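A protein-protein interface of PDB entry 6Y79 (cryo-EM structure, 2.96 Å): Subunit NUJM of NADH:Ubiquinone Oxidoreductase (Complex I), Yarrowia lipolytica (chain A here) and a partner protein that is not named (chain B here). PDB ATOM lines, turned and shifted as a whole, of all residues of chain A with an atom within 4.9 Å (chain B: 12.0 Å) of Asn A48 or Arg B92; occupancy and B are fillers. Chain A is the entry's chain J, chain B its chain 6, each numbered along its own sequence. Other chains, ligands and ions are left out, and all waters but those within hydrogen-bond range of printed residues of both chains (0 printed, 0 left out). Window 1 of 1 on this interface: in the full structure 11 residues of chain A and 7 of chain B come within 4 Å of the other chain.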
ATOM      1  N   ALA A  44      13.056  26.058 -13.225  1.00  0.00           N
ATOM      2  CA  ALA A  44      14.232  25.317 -12.784  1.00  0.00           C
ATOM      3  C   ALA A  44      14.244  23.910 -13.365  1.00  0.00           C
ATOM      4  O   ALA A  44      15.302  23.415 -13.777  1.00  0.00           O
ATOM      5  CB  ALA A  44      14.285  25.276 -11.259  1.00  0.00           C
ATOM      6  N   ALA A  45      13.068  23.271 -13.444  1.00  0.00           N
ATOM      7  CA  ALA A  45      12.968  21.975 -14.111  1.00  0.00           C
ATOM      8  C   ALA A  45      13.298  22.083 -15.596  1.00  0.00           C
ATOM      9  O   ALA A  45      13.937  21.186 -16.166  1.00  0.00           O
ATOM     10  CB  ALA A  45      11.569  21.400 -13.909  1.00  0.00           C
ATOM     11  N   ALA A  46      12.898  23.190 -16.226  1.00  0.00           N
ATOM     12  CA  ALA A  46      13.176  23.394 -17.646  1.00  0.00           C
ATOM     13  C   ALA A  46      14.661  23.605 -17.909  1.00  0.00           C
ATOM     14  O   ALA A  46      15.193  23.117 -18.912  1.00  0.00           O
ATOM     15  CB  ALA A  46      12.373  24.583 -18.161  1.00  0.00           C
ATOM     16  N   ARG A  47      15.345  24.333 -17.027  1.00  0.00           N
ATOM     17  CA  ARG A  47      16.784  24.518 -17.188  1.00  0.00           C
ATOM     18  C   ARG A  47      17.547  23.239 -16.889  1.00  0.00           C
ATOM     19  O   ARG A  47      18.622  23.011 -17.456  1.00  0.00           O
ATOM     20  CB  ARG A  47      17.280  25.625 -16.277  1.00  0.00           C
ATOM     21  CG  ARG A  47      16.681  26.948 -16.559  1.00  0.00           C
ATOM     22  CD  ARG A  47      17.257  27.934 -15.603  1.00  0.00           C
ATOM     23  NE  ARG A  47      18.702  27.980 -15.731  1.00  0.00           N
ATOM     24  CZ  ARG A  47      19.366  29.070 -16.083  1.00  0.00           C
ATOM     25  NH1 ARG A  47      18.699  30.184 -16.337  1.00  0.00           N
ATOM     26  NH2 ARG A  47      20.687  29.047 -16.183  1.00  0.00           N
ATOM     27  N   ASN A  48      17.036  22.426 -15.961  1.00  0.00           N
ATOM     28  CA  ASN A  48      17.621  21.117 -15.703  1.00  0.00           C
ATOM     29  C   ASN A  48      17.551  20.236 -16.940  1.00  0.00           C
ATOM     30  O   ASN A  48      18.557  19.657 -17.367  1.00  0.00           O
ATOM     31  CB  ASN A  48      16.902  20.451 -14.535  1.00  0.00           C
ATOM     32  CG  ASN A  48      17.621  19.218 -14.045  1.00  0.00           C
ATOM     33  OD1 ASN A  48      18.796  19.013 -14.337  1.00  0.00           O
ATOM     34  ND2 ASN A  48      16.909  18.375 -13.314  1.00  0.00           N
ATOM     35  N   SER A  49      16.359  20.132 -17.531  1.00  0.00           N
ATOM     36  CA  SER A  49      16.162  19.266 -18.685  1.00  0.00           C
ATOM     37  C   SER A  49      16.890  19.763 -19.926  1.00  0.00           C
ATOM     38  O   SER A  49      17.285  18.950 -20.764  1.00  0.00           O
ATOM     39  CB  SER A  49      14.673  19.134 -18.979  1.00  0.00           C
ATOM     40  OG  SER A  49      13.992  18.546 -17.885  1.00  0.00           O
ATOM     41  N   LEU A  50      17.056  21.073 -20.072  1.00  0.00           N
ATOM     42  CA  LEU A  50      17.722  21.643 -21.244  1.00  0.00           C
ATOM     43  C   LEU A  50      19.140  22.075 -20.882  1.00  0.00           C
ATOM     44  O   LEU A  50      19.452  23.261 -20.795  1.00  0.00           O
ATOM     45  CB  LEU A  50      16.913  22.816 -21.790  1.00  0.00           C
ATOM     46  CG  LEU A  50      15.791  22.588 -22.799  1.00  0.00           C
ATOM     47  CD1 LEU A  50      14.665  21.780 -22.211  1.00  0.00           C
ATOM     48  CD2 LEU A  50      15.270  23.921 -23.252  1.00  0.00           C
ATOM     49  N   ALA A  51      20.019  21.090 -20.712  1.00  0.00           N
ATOM     50  CA  ALA A  51      21.384  21.383 -20.298  1.00  0.00           C
ATOM     51  C   ALA A  51      22.290  20.218 -20.668  1.00  0.00           C
ATOM     52  O   ALA A  51      21.840  19.180 -21.156  1.00  0.00           O
ATOM     53  CB  ALA A  51      21.469  21.673 -18.797  1.00  0.00           C
ATOM     54  N   THR A  52      23.582  20.414 -20.423  1.00  0.00           N
ATOM     55  CA  THR A  52      24.636  19.435 -20.639  1.00  0.00           C
ATOM     56  C   THR A  52      25.259  19.108 -19.276  1.00  0.00           C
ATOM     57  O   THR A  52      24.940  19.730 -18.260  1.00  0.00           O
ATOM     58  CB  THR A  52      25.645  19.999 -21.654  1.00  0.00           C
ATOM     59  OG1 THR A  52      24.923  20.726 -22.656  1.00  0.00           O
ATOM     60  CG2 THR A  52      26.449  18.903 -22.375  1.00  0.00           C
ATOM     61  N   GLY A  53      26.132  18.105 -19.249  1.00  0.00           N
ATOM     62  CA  GLY A  53      26.951  17.831 -18.094  1.00  0.00           C
ATOM     63  C   GLY A  53      26.328  16.847 -17.128  1.00  0.00           C
ATOM     64  O   GLY A  53      25.204  16.373 -17.325  1.00  0.00           O
ATOM     65  N   ARG A  55      24.150  16.035 -14.509  1.00  0.00           N
ATOM     66  CA  ARG A  55      23.024  16.654 -13.829  1.00  0.00           C
ATOM     67  C   ARG A  55      22.095  15.576 -13.298  1.00  0.00           C
ATOM     68  O   ARG A  55      21.793  14.604 -13.995  1.00  0.00           O
ATOM     69  CB  ARG A  55      22.271  17.599 -14.756  1.00  0.00           C
ATOM     70  CG  ARG A  55      22.948  18.944 -14.889  1.00  0.00           C
ATOM     71  CD  ARG A  55      22.019  19.969 -15.473  1.00  0.00           C
ATOM     72  NE  ARG A  55      22.641  21.286 -15.544  1.00  0.00           N
ATOM     73  CZ  ARG A  55      22.211  22.351 -14.879  1.00  0.00           C
ATOM     74  NH1 ARG A  55      22.839  23.509 -15.010  1.00  0.00           N
ATOM     75  NH2 ARG A  55      21.148  22.260 -14.096  1.00  0.00           N
ATOM     76  N   ASN A  56      21.652  15.757 -12.058  1.00  0.00           N
ATOM     77  CA  ASN A  56      20.831  14.775 -11.364  1.00  0.00           C
ATOM     78  C   ASN A  56      19.548  15.440 -10.882  1.00  0.00           C
ATOM     79  O   ASN A  56      19.171  16.497 -11.389  1.00  0.00           O
ATOM     80  CB  ASN A  56      21.604  14.107 -10.214  1.00  0.00           C
ATOM     81  CG  ASN A  56      22.172  15.092  -9.201  1.00  0.00           C
ATOM     82  OD1 ASN A  56      21.967  16.298  -9.279  1.00  0.00           O
ATOM     83  ND2 ASN A  56      22.890  14.559  -8.223  1.00  0.00           N
ATOM     84  N   ILE A  57      18.827  14.808  -9.959  1.00  0.00           N
ATOM     85  CA  ILE A  57      17.519  15.335  -9.594  1.00  0.00           C
ATOM     86  C   ILE A  57      17.629  16.511  -8.622  1.00  0.00           C
ATOM     87  O   ILE A  57      16.774  17.411  -8.634  1.00  0.00           O
ATOM     88  CB  ILE A  57      16.646  14.187  -9.054  1.00  0.00           C
ATOM     89  CG1 ILE A  57      15.222  14.631  -8.713  1.00  0.00           C
ATOM     90  CG2 ILE A  57      17.356  13.397  -7.967  1.00  0.00           C
ATOM     91  CD1 ILE A  57      14.184  13.559  -8.903  1.00  0.00           C
ATOM     92  N   THR A  59      20.318  18.705  -8.508  1.00  0.00           N
ATOM     93  CA  THR A  59      20.971  19.868  -9.109  1.00  0.00           C
ATOM     94  C   THR A  59      19.961  20.871  -9.658  1.00  0.00           C
ATOM     95  O   THR A  59      20.359  21.924 -10.167  1.00  0.00           O
ATOM     96  CB  THR A  59      21.934  19.456 -10.230  1.00  0.00           C
ATOM     97  OG1 THR A  59      22.772  20.568 -10.568  1.00  0.00           O
ATOM     98  CG2 THR A  59      21.176  19.055 -11.468  1.00  0.00           C
ATOM     99  N   THR A  60      18.667  20.556  -9.546  1.00  0.00           N
ATOM    100  CA  THR A  60      17.615  21.473  -9.969  1.00  0.00           C
ATOM    101  C   THR A  60      17.609  22.736  -9.110  1.00  0.00           C
ATOM    102  O   THR A  60      17.254  23.815  -9.589  1.00  0.00           O
ATOM    103  CB  THR A  60      16.262  20.749  -9.913  1.00  0.00           C
ATOM    104  OG1 THR A  60      16.342  19.535 -10.668  1.00  0.00           O
ATOM    105  CG2 THR A  60      15.139  21.590 -10.499  1.00  0.00           C
ATOM    106  N   THR B  83      21.922   4.526 -26.820  1.00  0.00           N
ATOM    107  CA  THR B  83      22.243   4.455 -25.405  1.00  0.00           C
ATOM    108  C   THR B  83      21.068   3.800 -24.697  1.00  0.00           C
ATOM    109  O   THR B  83      19.931   3.886 -25.160  1.00  0.00           O
ATOM    110  CB  THR B  83      22.511   5.844 -24.816  1.00  0.00           C
ATOM    111  OG1 THR B  83      21.273   6.477 -24.468  1.00  0.00           O
ATOM    112  CG2 THR B  83      23.239   6.719 -25.813  1.00  0.00           C
ATOM    113  N   GLU B  84      21.336   3.096 -23.607  1.00  0.00           N
ATOM    114  CA  GLU B  84      20.183   2.591 -22.886  1.00  0.00           C
ATOM    115  C   GLU B  84      19.856   3.528 -21.726  1.00  0.00           C
ATOM    116  O   GLU B  84      20.628   4.424 -21.383  1.00  0.00           O
ATOM    117  CB  GLU B  84      20.401   1.152 -22.408  1.00  0.00           C
ATOM    118  CG  GLU B  84      19.090   0.364 -22.404  1.00  0.00           C
ATOM    119  CD  GLU B  84      19.219  -1.050 -21.953  1.00  0.00           C
ATOM    120  OE1 GLU B  84      18.215  -1.577 -21.415  1.00  0.00           O
ATOM    121  OE2 GLU B  84      20.285  -1.669 -22.163  1.00  0.00           O
ATOM    122  N   LEU B  85      18.702   3.285 -21.103  1.00  0.00           N
ATOM    123  CA  LEU B  85      18.109   4.166 -20.106  1.00  0.00           C
ATOM    124  C   LEU B  85      18.974   4.137 -18.852  1.00  0.00           C
ATOM    125  O   LEU B  85      18.693   3.448 -17.869  1.00  0.00           O
ATOM    126  CB  LEU B  85      16.676   3.737 -19.799  1.00  0.00           C
ATOM    127  CG  LEU B  85      15.826   4.745 -19.015  1.00  0.00           C
ATOM    128  CD1 LEU B  85      15.581   5.934 -19.897  1.00  0.00           C
ATOM    129  CD2 LEU B  85      14.520   4.123 -18.567  1.00  0.00           C
ATOM    130  N   SER B  86      20.072   4.878 -18.920  1.00  0.00           N
ATOM    131  CA  SER B  86      20.854   5.176 -17.747  1.00  0.00           C
ATOM    132  C   SER B  86      20.030   6.068 -16.846  1.00  0.00           C
ATOM    133  O   SER B  86      19.147   6.808 -17.293  1.00  0.00           O
ATOM    134  CB  SER B  86      22.161   5.870 -18.131  1.00  0.00           C
ATOM    135  OG  SER B  86      22.816   5.187 -19.194  1.00  0.00           O
ATOM    136  N   VAL B  87      20.318   5.970 -15.557  1.00  0.00           N
ATOM    137  CA  VAL B  87      19.658   6.822 -14.581  1.00  0.00           C
ATOM    138  C   VAL B  87      20.405   8.163 -14.465  1.00  0.00           C
ATOM    139  O   VAL B  87      19.817   9.211 -14.128  1.00  0.00           O
ATOM    140  CB  VAL B  87      19.553   6.017 -13.267  1.00  0.00           C
ATOM    141  CG1 VAL B  87      20.945   5.746 -12.664  1.00  0.00           C
ATOM    142  CG2 VAL B  87      18.566   6.675 -12.254  1.00  0.00           C
ATOM    143  N   LYS B  88      21.698   8.147 -14.809  1.00  0.00           N
ATOM    144  CA  LYS B  88      22.516   9.348 -14.884  1.00  0.00           C
ATOM    145  C   LYS B  88      22.075  10.252 -16.018  1.00  0.00           C
ATOM    146  O   LYS B  88      22.330  11.458 -15.966  1.00  0.00           O
ATOM    147  CB  LYS B  88      23.991   8.968 -15.067  1.00  0.00           C
ATOM    148  CG  LYS B  88      24.318   8.292 -16.415  1.00  0.00           C
ATOM    149  CD  LYS B  88      25.772   7.895 -16.589  1.00  0.00           C
ATOM    150  CE  LYS B  88      26.616   9.069 -17.032  1.00  0.00           C
ATOM    151  NZ  LYS B  88      27.943   8.623 -17.525  1.00  0.00           N
ATOM    152  N   SER B  89      21.425   9.693 -17.044  1.00  0.00           N
ATOM    153  CA  SER B  89      21.079  10.450 -18.233  1.00  0.00           C
ATOM    154  C   SER B  89      19.740  11.149 -18.088  1.00  0.00           C
ATOM    155  O   SER B  89      19.550  12.230 -18.656  1.00  0.00           O
ATOM    156  CB  SER B  89      21.021   9.537 -19.458  1.00  0.00           C
ATOM    157  OG  SER B  89      22.248   8.849 -19.702  1.00  0.00           O
ATOM    158  N   ASN B  90      18.804  10.558 -17.340  1.00  0.00           N
ATOM    159  CA  ASN B  90      17.393  10.863 -17.511  1.00  0.00           C
ATOM    160  C   ASN B  90      16.640  11.264 -16.247  1.00  0.00           C
ATOM    161  O   ASN B  90      15.443  11.562 -16.340  1.00  0.00           O
ATOM    162  CB  ASN B  90      16.689   9.665 -18.155  1.00  0.00           C
ATOM    163  CG  ASN B  90      17.082   9.471 -19.628  1.00  0.00           C
ATOM    164  OD1 ASN B  90      17.792   8.531 -19.978  1.00  0.00           O
ATOM    165  ND2 ASN B  90      16.592  10.355 -20.495  1.00  0.00           N
ATOM    166  N   ILE B  91      17.267  11.253 -15.065  1.00  0.00           N
ATOM    167  CA  ILE B  91      16.571  11.837 -13.907  1.00  0.00           C
ATOM    168  C   ILE B  91      16.866  13.348 -13.814  1.00  0.00           C
ATOM    169  O   ILE B  91      16.187  14.085 -13.084  1.00  0.00           O
ATOM    170  CB  ILE B  91      16.816  10.971 -12.628  1.00  0.00           C
ATOM    171  CG1 ILE B  91      16.045   9.641 -12.808  1.00  0.00           C
ATOM    172  CG2 ILE B  91      16.249  11.526 -11.372  1.00  0.00           C
ATOM    173  CD1 ILE B  91      15.545   8.805 -11.503  1.00  0.00           C
ATOM    174  N   ARG B  92      17.754  13.866 -14.667  1.00  0.00           N
ATOM    175  CA  ARG B  92      17.739  15.305 -14.900  1.00  0.00           C
ATOM    176  C   ARG B  92      16.483  15.728 -15.645  1.00  0.00           C
ATOM    177  O   ARG B  92      16.033  16.867 -15.481  1.00  0.00           O
ATOM    178  CB  ARG B  92      18.988  15.779 -15.654  1.00  0.00           C
ATOM    179  CG  ARG B  92      19.080  15.481 -17.127  1.00  0.00           C
ATOM    180  CD  ARG B  92      20.325  16.148 -17.640  1.00  0.00           C
ATOM    181  NE  ARG B  92      20.582  15.887 -19.042  1.00  0.00           N
ATOM    182  CZ  ARG B  92      21.623  16.389 -19.691  1.00  0.00           C
ATOM    183  NH1 ARG B  92      21.814  16.114 -20.971  1.00  0.00           N
ATOM    184  NH2 ARG B  92      22.474  17.172 -19.045  1.00  0.00           N
ATOM    185  N   ASP B  93      15.870  14.810 -16.395  1.00  0.00           N
ATOM    186  CA  ASP B  93      14.617  15.081 -17.082  1.00  0.00           C
ATOM    187  C   ASP B  93      13.400  15.031 -16.158  1.00  0.00           C
ATOM    188  O   ASP B  93      12.497  15.856 -16.316  1.00  0.00           O
ATOM    189  CB  ASP B  93      14.450  14.088 -18.225  1.00  0.00           C
ATOM    190  CG  ASP B  93      15.446  14.320 -19.333  1.00  0.00           C
ATOM    191  OD1 ASP B  93      15.898  15.476 -19.482  1.00  0.00           O
ATOM    192  OD2 ASP B  93      15.781  13.362 -20.060  1.00  0.00           O
ATOM    193  N   LEU B  94      13.373  14.114 -15.170  1.00  0.00           N
ATOM    194  CA  LEU B  94      12.191  13.751 -14.368  1.00  0.00           C
ATOM    195  C   LEU B  94      11.356  14.850 -13.687  1.00  0.00           C
ATOM    196  O   LEU B  94      10.130  14.675 -13.624  1.00  0.00           O
ATOM    197  CB  LEU B  94      12.594  12.727 -13.296  1.00  0.00           C
ATOM    198  CG  LEU B  94      11.439  11.933 -12.647  1.00  0.00           C
ATOM    199  CD1 LEU B  94      10.831  10.913 -13.608  1.00  0.00           C
ATOM    200  CD2 LEU B  94      11.839  11.271 -11.334  1.00  0.00           C
ATOM    201  N   PRO B  95      11.902  15.964 -13.157  1.00  0.00           N
ATOM    202  CA  PRO B  95      10.982  16.971 -12.584  1.00  0.00           C
ATOM    203  C   PRO B  95      10.091  17.636 -13.621  1.00  0.00           C
ATOM    204  O   PRO B  95       8.882  17.788 -13.383  1.00  0.00           O
ATOM    205  CB  PRO B  95      11.927  17.974 -11.907  1.00  0.00           C
ATOM    206  CG  PRO B  95      13.202  17.821 -12.610  1.00  0.00           C
ATOM    207  CD  PRO B  95      13.303  16.360 -12.903  1.00  0.00           C
ATOM    208  N   LEU B  96      10.629  17.955 -14.799  1.00  0.00           N
ATOM    209  CA  LEU B  96       9.771  18.484 -15.848  1.00  0.00           C
ATOM    210  C   LEU B  96       8.898  17.393 -16.456  1.00  0.00           C
ATOM    211  O   LEU B  96       7.795  17.694 -16.915  1.00  0.00           O
ATOM    212  CB  LEU B  96      10.598  19.183 -16.928  1.00  0.00           C
ATOM    213  CG  LEU B  96       9.797  20.070 -17.889  1.00  0.00           C
ATOM    214  CD1 LEU B  96       8.953  21.096 -17.139  1.00  0.00           C
ATOM    215  CD2 LEU B  96      10.715  20.756 -18.862  1.00  0.00           C
ATOM    216  N   VAL B  97       9.349  16.130 -16.436  1.00  0.00           N
ATOM    217  CA  VAL B  97       8.491  15.021 -16.868  1.00  0.00           C
ATOM    218  C   VAL B  97       7.266  14.922 -15.970  1.00  0.00           C
ATOM    219  O   VAL B  97       6.143  14.765 -16.448  1.00  0.00           O
ATOM    220  CB  VAL B  97       9.256  13.683 -16.886  1.00  0.00           C
ATOM    221  CG1 VAL B  97       8.359  12.579 -17.399  1.00  0.00           C
ATOM    222  CG2 VAL B  97      10.476  13.750 -17.749  1.00  0.00           C
ATOM    223  N   LEU B  98       7.464  15.057 -14.660  1.00  0.00           N
ATOM    224  CA  LEU B  98       6.351  14.961 -13.720  1.00  0.00           C
ATOM    225  C   LEU B  98       5.400  16.148 -13.852  1.00  0.00           C
ATOM    226  O   LEU B  98       4.171  15.964 -13.881  1.00  0.00           O
ATOM    227  CB  LEU B  98       6.891  14.855 -12.296  1.00  0.00           C
ATOM    228  CG  LEU B  98       5.847  14.661 -11.206  1.00  0.00           C
ATOM    229  CD1 LEU B  98       5.096  13.358 -11.412  1.00  0.00           C
ATOM    230  CD2 LEU B  98       6.510  14.686  -9.848  1.00  0.00           C
ATOM    231  N   ILE B  99       5.956  17.364 -13.961  1.00  0.00           N
ATOM    232  CA  ILE B  99       5.133  18.569 -14.105  1.00  0.00           C
ATOM    233  C   ILE B  99       4.344  18.530 -15.407  1.00  0.00           C
ATOM    234  O   ILE B  99       3.132  18.776 -15.424  1.00  0.00           O
ATOM    235  CB  ILE B  99       6.004  19.835 -14.023  1.00  0.00           C
ATOM    236  CG1 ILE B  99       6.599  19.986 -12.628  1.00  0.00           C
ATOM    237  CG2 ILE B  99       5.191  21.073 -14.349  1.00  0.00           C
ATOM    238  CD1 ILE B  99       7.695  21.011 -12.560  1.00  0.00           C
ATOM    239  N   SER B 100       5.007  18.171 -16.508  1.00  0.00           N
ATOM    240  CA  SER B 100       4.335  18.106 -17.794  1.00  0.00           C
ATOM    241  C   SER B 100       3.371  16.932 -17.877  1.00  0.00           C
ATOM    242  O   SER B 100       2.360  17.044 -18.561  1.00  0.00           O
ATOM    243  CB  SER B 100       5.366  18.025 -18.910  1.00  0.00           C
ATOM    244  OG  SER B 100       5.789  16.689 -19.089  1.00  0.00           O
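Among the printed residues, merely in contact across the chains: Ala A45 with Pro B95 (3.98 Å), Ala A45 with Leu B96 (3.7 Å), Ala A46 with Leu B96 (3.8 Å), Asn A48 with Pro B95 (3.8 Å), Ser A49 with Arg B92 (3.6 Å), Ser A49 with Leu B96 (3.6 Å), Thr A52 with Arg B92 (3.4 Å), Arg A55 with Lys B88 (3.8 Å), Arg A55 with Arg B92 (3.5 Å), Asn A56 with Arg B92 (3.97 Å) and Ile A57 with Ile B91 (3.6 Å).
O of Leu B96 is in hydrogen-bond range of OG of Ser B100. ND2 of Asn A48 is in hydrogen-bond range of OG1 of Thr A60 (2.9 Å). The backbone NH of Thr A59 sits at hydrogen-bond distance from the side-chain amide oxygen of Asn A56 (3.0 Å). The side-chain hydroxyl (OG1) of Thr A60 lies within hydrogen-bond range of the backbone carbonyl oxygen (O) of Ile A57 (3.0 Å). OD2 of Asp B93 sits at hydrogen-bond distance from ND2 of Asn B90 (3.1 Å). O of Ala A45 sits at hydrogen-bond distance from OG of Ser A49.
The backbone carbonyl oxygen (O) of Arg B92 is in hydrogen-bond range of the side-chain amide nitrogen (ND2) of Asn A48 (2.8 Å). The backbone carbonyl oxygen of Asp B93 sits at hydrogen-bond distance from the side-chain hydroxyl of Ser A49. The guanidinium group of Arg B92 sits at hydrogen-bond distance from the backbone carbonyl oxygen of Ala A51, 3.0 Å away. NH2 of Arg B92 is in hydrogen-bond range of O of Gly A53 (3.3 Å).
Hydrophobic or aromatic side chains of chain A that line the printed part of chain B: Ala A45 and Ile A57. Of the 18 printed residues of chain B, 6 touch a printed residue of chain A. Hydrophobic or aromatic side chains of chain B that line the printed part of chain A: Ile B91, Pro B95 and Leu B96. Along chain B the printed residues that touch a printed residue of chain A span positions 88 to 96. Among the printed residues, no Asp or Glu carboxylate lies within 4 Å of a Lys or Arg side-chain nitrogen of the other chain.
Of chain B, only Arg B92 (2.8 Å) and Pro B95 (3.8 Å) come within 4 Å of Asn A48. Arg B92 touches seven residues of chain A. No residue of chain B comes within 4 Å of Ala A44. Ala A46 touches just one residue of chain B: Leu B96 (3.8 Å). No residue of chain B comes within 4 Å of Arg A47. Of chain B, only Arg B92 (3.6 Å), Asp B93 (3.5 Å) and Leu B96 (3.6 Å) come within 4 Å of Ser A49. No residue of chain B comes within 4 Å of Leu A50. Thr A52 touches just one residue of chain B: Arg B92. Of the printed residues of chain B, Gly A53 touches Arg B92 (3.3 Å). Arg A55 touches just these residues of chain B: Lys B88 and Arg B92. Of the printed residues of chain B, Ile A57 touches Ile B91 (3.6 Å). No residue of chain B comes within 4 Å of Thr A59. Thr A60 touches none of the printed residues of chain B. Of the printed residues of chain A, Ile B91 touches Ile A57 (3.6 Å). Printed residues of chain A within 4 Å of Leu B96: Ala A45 (3.7 Å), Ala A46 (3.8 Å) and Ser A49 (3.6 Å). Of the printed residues of chain B, Asn A56 touches Arg B92. Of the printed residues of chain A, Pro B95 touches Ala A45 and Asn A48. Printed residues of chain B within 4 Å of Ala A45: Pro B95 and Leu B96. Ser B89 touches none of the printed residues of chain A. Ser B100 touches none of the printed residues of chain A. The nearest residue of chain B that does not touch Asn A48 is Ile B91 (4.4 Å).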
